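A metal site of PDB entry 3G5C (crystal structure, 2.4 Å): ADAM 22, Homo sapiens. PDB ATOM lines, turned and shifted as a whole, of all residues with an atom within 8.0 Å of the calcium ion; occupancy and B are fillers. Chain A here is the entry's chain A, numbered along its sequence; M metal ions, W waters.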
ATOM      1  N   TYR A   8     -16.437 -11.770 -20.617  1.00  0.00           N
ATOM      2  CA  TYR A   8     -16.535 -13.113 -21.180  1.00  0.00           C
ATOM      3  C   TYR A   8     -15.905 -13.208 -22.568  1.00  0.00           C
ATOM      4  O   TYR A   8     -16.386 -12.597 -23.527  1.00  0.00           O
ATOM      5  CB  TYR A   8     -17.998 -13.607 -21.274  1.00  0.00           C
ATOM      6  CG  TYR A   8     -18.776 -13.524 -19.976  1.00  0.00           C
ATOM      7  CD1 TYR A   8     -19.302 -12.309 -19.549  1.00  0.00           C
ATOM      8  CD2 TYR A   8     -18.964 -14.651 -19.167  1.00  0.00           C
ATOM      9  CE1 TYR A   8     -19.973 -12.198 -18.333  1.00  0.00           C
ATOM     10  CE2 TYR A   8     -19.640 -14.550 -17.943  1.00  0.00           C
ATOM     11  CZ  TYR A   8     -20.143 -13.318 -17.530  1.00  0.00           C
ATOM     12  OH  TYR A   8     -20.790 -13.179 -16.313  1.00  0.00           O
ATOM     13  N   ILE A   9     -14.815 -13.959 -22.646  1.00  0.00           N
ATOM     14  CA  ILE A   9     -14.120 -14.159 -23.909  1.00  0.00           C
ATOM     15  C   ILE A   9     -14.614 -15.439 -24.600  1.00  0.00           C
ATOM     16  O   ILE A   9     -14.256 -16.543 -24.212  1.00  0.00           O
ATOM     17  CB  ILE A   9     -12.609 -14.282 -23.712  1.00  0.00           C
ATOM     18  CG1 ILE A   9     -12.063 -13.067 -22.963  1.00  0.00           C
ATOM     19  CG2 ILE A   9     -11.968 -14.307 -25.066  1.00  0.00           C
ATOM     20  CD1 ILE A   9     -10.663 -13.269 -22.390  1.00  0.00           C
ATOM     21  N   GLU A  10     -15.479 -15.253 -25.601  1.00  0.00           N
ATOM     22  CA  GLU A  10     -15.958 -16.353 -26.431  1.00  0.00           C
ATOM     23  C   GLU A  10     -14.801 -16.772 -27.327  1.00  0.00           C
ATOM     24  O   GLU A  10     -14.407 -16.048 -28.237  1.00  0.00           O
ATOM     25  CB  GLU A  10     -17.176 -15.915 -27.253  1.00  0.00           C
ATOM     26  CG  GLU A  10     -18.509 -15.848 -26.462  1.00  0.00           C
ATOM     27  CD  GLU A  10     -19.592 -15.050 -27.193  1.00  0.00           C
ATOM     28  OE1 GLU A  10     -20.787 -15.146 -26.833  1.00  0.00           O
ATOM     29  OE2 GLU A  10     -19.224 -14.299 -28.121  1.00  0.00           O
ATOM     30  N   LEU A  11     -14.275 -17.974 -27.057  1.00  0.00           N
ATOM     31  CA  LEU A  11     -13.056 -18.425 -27.706  1.00  0.00           C
ATOM     32  C   LEU A  11     -13.227 -19.620 -28.630  1.00  0.00           C
ATOM     33  O   LEU A  11     -13.933 -20.578 -28.309  1.00  0.00           O
ATOM     34  CB  LEU A  11     -12.007 -18.725 -26.633  1.00  0.00           C
ATOM     35  CG  LEU A  11     -10.718 -19.479 -27.005  1.00  0.00           C
ATOM     36  CD1 LEU A  11      -9.876 -18.632 -27.911  1.00  0.00           C
ATOM     37  CD2 LEU A  11      -9.946 -19.814 -25.742  1.00  0.00           C
ATOM     38  N   VAL A  56     -16.395 -21.596 -27.226  1.00  0.00           N
ATOM     39  CA  VAL A  56     -17.654 -21.605 -27.977  1.00  0.00           C
ATOM     40  C   VAL A  56     -17.617 -22.465 -29.241  1.00  0.00           C
ATOM     41  O   VAL A  56     -18.642 -22.984 -29.660  1.00  0.00           O
ATOM     42  CB  VAL A  56     -18.135 -20.152 -28.331  1.00  0.00           C
ATOM     43  CG1 VAL A  56     -18.347 -19.367 -27.069  1.00  0.00           C
ATOM     44  CG2 VAL A  56     -17.116 -19.432 -29.194  1.00  0.00           C
ATOM     45  N   LYS A  91     -18.846 -17.580 -34.969  1.00  0.00           N
ATOM     46  CA  LYS A  91     -18.724 -16.336 -34.204  1.00  0.00           C
ATOM     47  C   LYS A  91     -17.936 -16.517 -32.908  1.00  0.00           C
ATOM     48  O   LYS A  91     -18.250 -17.387 -32.096  1.00  0.00           O
ATOM     49  CB  LYS A  91     -20.105 -15.784 -33.870  1.00  0.00           C
ATOM     50  CG  LYS A  91     -20.857 -15.320 -35.083  1.00  0.00           C
ATOM     51  CD  LYS A  91     -20.070 -14.261 -35.819  1.00  0.00           C
ATOM     52  CE  LYS A  91     -20.839 -13.779 -37.031  1.00  0.00           C
ATOM     53  NZ  LYS A  91     -20.139 -12.652 -37.698  1.00  0.00           N
ATOM     54  N   SER A  92     -16.913 -15.676 -32.738  1.00  0.00           N
ATOM     55  CA  SER A  92     -16.067 -15.716 -31.557  1.00  0.00           C
ATOM     56  C   SER A  92     -15.362 -14.374 -31.325  1.00  0.00           C
ATOM     57  O   SER A  92     -15.132 -13.613 -32.261  1.00  0.00           O
ATOM     58  CB  SER A  92     -14.998 -16.815 -31.706  1.00  0.00           C
ATOM     59  OG  SER A  92     -14.123 -16.570 -32.796  1.00  0.00           O
ATOM     60  N   ASP A  93     -15.030 -14.103 -30.059  1.00  0.00           N
ATOM     61  CA  ASP A  93     -14.297 -12.901 -29.684  1.00  0.00           C
ATOM     62  C   ASP A  93     -12.814 -13.037 -30.068  1.00  0.00           C
ATOM     63  O   ASP A  93     -12.166 -12.048 -30.433  1.00  0.00           O
ATOM     64  CB  ASP A  93     -14.429 -12.671 -28.166  1.00  0.00           C
ATOM     65  CG  ASP A  93     -15.889 -12.431 -27.712  1.00  0.00           C
ATOM     66  OD1 ASP A  93     -16.178 -12.627 -26.510  1.00  0.00           O
ATOM     67  OD2 ASP A  93     -16.726 -12.044 -28.567  1.00  0.00           O
ATOM     68  N   ALA A  94     -12.288 -14.269 -29.990  1.00  0.00           N
ATOM     69  CA  ALA A  94     -10.900 -14.562 -30.346  1.00  0.00           C
ATOM     70  C   ALA A  94     -10.748 -15.983 -30.897  1.00  0.00           C
ATOM     71  O   ALA A  94     -11.402 -16.913 -30.426  1.00  0.00           O
ATOM     72  CB  ALA A  94      -9.979 -14.370 -29.147  1.00  0.00           C
ATOM     73  N   CYS A 117     -12.200  -8.752 -30.539  1.00  0.00           N
ATOM     74  CA  CYS A 117     -13.323  -8.160 -31.260  1.00  0.00           C
ATOM     75  C   CYS A 117     -13.010  -7.846 -32.733  1.00  0.00           C
ATOM     76  O   CYS A 117     -13.923  -7.608 -33.529  1.00  0.00           O
ATOM     77  CB  CYS A 117     -13.780  -6.904 -30.528  1.00  0.00           C
ATOM     78  SG  CYS A 117     -14.082  -7.109 -28.723  1.00  0.00           S
ATOM     79  N   GLY A 199     -12.593  -3.905 -26.201  1.00  0.00           N
ATOM     80  CA  GLY A 199     -13.218  -5.105 -25.675  1.00  0.00           C
ATOM     81  C   GLY A 199     -14.711  -5.007 -25.488  1.00  0.00           C
ATOM     82  O   GLY A 199     -15.252  -5.434 -24.465  1.00  0.00           O
ATOM     83  N   ALA A 200     -15.390  -4.440 -26.484  1.00  0.00           N
ATOM     84  CA  ALA A 200     -16.844  -4.274 -26.441  1.00  0.00           C
ATOM     85  C   ALA A 200     -17.593  -5.598 -26.594  1.00  0.00           C
ATOM     86  O   ALA A 200     -18.692  -5.771 -26.057  1.00  0.00           O
ATOM     87  CB  ALA A 200     -17.300  -3.291 -27.524  1.00  0.00           C
ATOM     88  N   CYS A 201     -16.994  -6.536 -27.318  1.00  0.00           N
ATOM     89  CA  CYS A 201     -17.590  -7.854 -27.565  1.00  0.00           C
ATOM     90  C   CYS A 201     -17.437  -8.810 -26.374  1.00  0.00           C
ATOM     91  O   CYS A 201     -17.919  -9.953 -26.411  1.00  0.00           O
ATOM     92  CB  CYS A 201     -16.867  -8.476 -28.759  1.00  0.00           C
ATOM     93  SG  CYS A 201     -15.089  -8.865 -28.519  1.00  0.00           S
ATOM     94  N   LEU A 202     -16.776  -8.339 -25.316  1.00  0.00           N
ATOM     95  CA  LEU A 202     -16.515  -9.149 -24.121  1.00  0.00           C
ATOM     96  C   LEU A 202     -17.575  -9.002 -23.037  1.00  0.00           C
ATOM     97  O   LEU A 202     -17.334  -9.373 -21.875  1.00  0.00           O
ATOM     98  CB  LEU A 202     -15.187  -8.681 -23.540  1.00  0.00           C
ATOM     99  CG  LEU A 202     -13.859  -9.433 -23.638  1.00  0.00           C
ATOM    100  CD1 LEU A 202     -13.618 -10.049 -25.007  1.00  0.00           C
ATOM    101  CD2 LEU A 202     -12.790  -8.425 -23.271  1.00  0.00           C
ATOM    102  N   PHE A 203     -18.747  -8.486 -23.391  1.00  0.00           N
ATOM    103  CA  PHE A 203     -19.792  -8.182 -22.405  1.00  0.00           C
ATOM    104  C   PHE A 203     -21.083  -8.979 -22.509  1.00  0.00           C
ATOM    105  O   PHE A 203     -22.015  -8.743 -21.745  1.00  0.00           O
ATOM    106  CB  PHE A 203     -20.097  -6.694 -22.434  1.00  0.00           C
ATOM    107  CG  PHE A 203     -19.051  -5.865 -21.788  1.00  0.00           C
ATOM    108  CD1 PHE A 203     -19.150  -5.512 -20.444  1.00  0.00           C
ATOM    109  CD2 PHE A 203     -17.923  -5.482 -22.489  1.00  0.00           C
ATOM    110  CE1 PHE A 203     -18.143  -4.780 -19.808  1.00  0.00           C
ATOM    111  CE2 PHE A 203     -16.899  -4.757 -21.876  1.00  0.00           C
ATOM    112  CZ  PHE A 203     -17.007  -4.406 -20.529  1.00  0.00           C
ATOM    113  N   ASN A 204     -21.138  -9.926 -23.444  1.00  0.00           N
ATOM    114  CA  ASN A 204     -22.291 -10.807 -23.547  1.00  0.00           C
ATOM    115  C   ASN A 204     -21.998 -12.194 -22.973  1.00  0.00           C
ATOM    116  O   ASN A 204     -20.905 -12.729 -23.129  1.00  0.00           O
ATOM    117  CB  ASN A 204     -22.762 -10.891 -25.009  1.00  0.00           C
ATOM    118  CG  ASN A 204     -21.764 -11.536 -25.906  1.00  0.00           C
ATOM    119  OD1 ASN A 204     -20.789 -10.916 -26.345  1.00  0.00           O
ATOM    120  ND2 ASN A 204     -21.987 -12.817 -26.190  1.00  0.00           N
ATOM    121  N   LYS A 205     -22.996 -12.757 -22.285  1.00  0.00           N
ATOM    122  CA  LYS A 205     -22.850 -14.076 -21.687  1.00  0.00           C
ATOM    123  C   LYS A 205     -23.311 -15.191 -22.609  1.00  0.00           C
ATOM    124  O   LYS A 205     -24.437 -15.159 -23.126  1.00  0.00           O
ATOM    125  CB  LYS A 205     -23.614 -14.193 -20.376  1.00  0.00           C
ATOM    126  CG  LYS A 205     -22.936 -13.529 -19.215  1.00  0.00           C
ATOM    127  CD  LYS A 205     -23.615 -13.907 -17.900  1.00  0.00           C
ATOM    128  CE  LYS A 205     -23.429 -15.374 -17.521  1.00  0.00           C
ATOM    129  NZ  LYS A 205     -23.950 -15.657 -16.142  1.00  0.00           N
ATOM    130  N   PRO A 206     -22.431 -16.179 -22.851  1.00  0.00           N
ATOM    131  CA  PRO A 206     -22.775 -17.361 -23.656  1.00  0.00           C
ATOM    132  C   PRO A 206     -23.787 -18.246 -22.895  1.00  0.00           C
ATOM    133  O   PRO A 206     -23.942 -18.121 -21.674  1.00  0.00           O
ATOM    134  CB  PRO A 206     -21.439 -18.076 -23.822  1.00  0.00           C
ATOM    135  CG  PRO A 206     -20.420 -17.017 -23.553  1.00  0.00           C
ATOM    136  CD  PRO A 206     -21.019 -16.238 -22.428  1.00  0.00           C
ATOM    137  N   PRO A 293     -25.903  -6.296 -25.112  1.00  0.00           N
ATOM    138  CA  PRO A 293     -24.540  -6.396 -25.652  1.00  0.00           C
ATOM    139  C   PRO A 293     -23.896  -5.029 -25.865  1.00  0.00           C
ATOM    140  O   PRO A 293     -24.487  -4.164 -26.515  1.00  0.00           O
ATOM    141  CB  PRO A 293     -24.750  -7.054 -27.024  1.00  0.00           C
ATOM    142  CG  PRO A 293     -26.083  -7.721 -26.934  1.00  0.00           C
ATOM    143  CD  PRO A 293     -26.898  -6.779 -26.092  1.00  0.00           C
HETATM  144 CA    CA M   1     -18.704 -11.908 -27.074  1.00  0.00          CA
HETATM  145  O   HOH W   1     -18.619 -12.861 -25.108  1.00  0.00           O
HETATM  146  O   HOH W   2     -19.777 -11.404 -28.997  1.00  0.00           O
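O of Asp 93 is in hydrogen-bond range of N of Cys 117 (3.3 Å).
The side-chain sulfur (SG) of Cys 117 forms a disulfide with the side-chain sulfur (SG) of Cys 201.
The backbone NH of Ala 94 is in hydrogen-bond range of the backbone carbonyl oxygen of Glu 10, at 3.3 Å.
Water W1 lies within hydrogen-bond range of O of Tyr 8 and O of Asn 204.
The calcium ion is bound by water W1 (2.2 Å), the backbone carbonyl oxygen (O) of Cys 201 (2.2 Å), water W2 (2.3 Å), the side-chain amide oxygen (OD1) of Asn 204 (2.4 Å), the side-chain carboxylate (OD2) of Asp 93 (2.5 Å), the side-chain carboxylate (OE2) of Glu 10 (2.7 Å) and the side-chain carboxylate (OD1) of Asp 93 (2.7 Å).
Within 4 Å of the calcium ion: Glu 10, Asp 93, Cys 201 and Asn 204.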
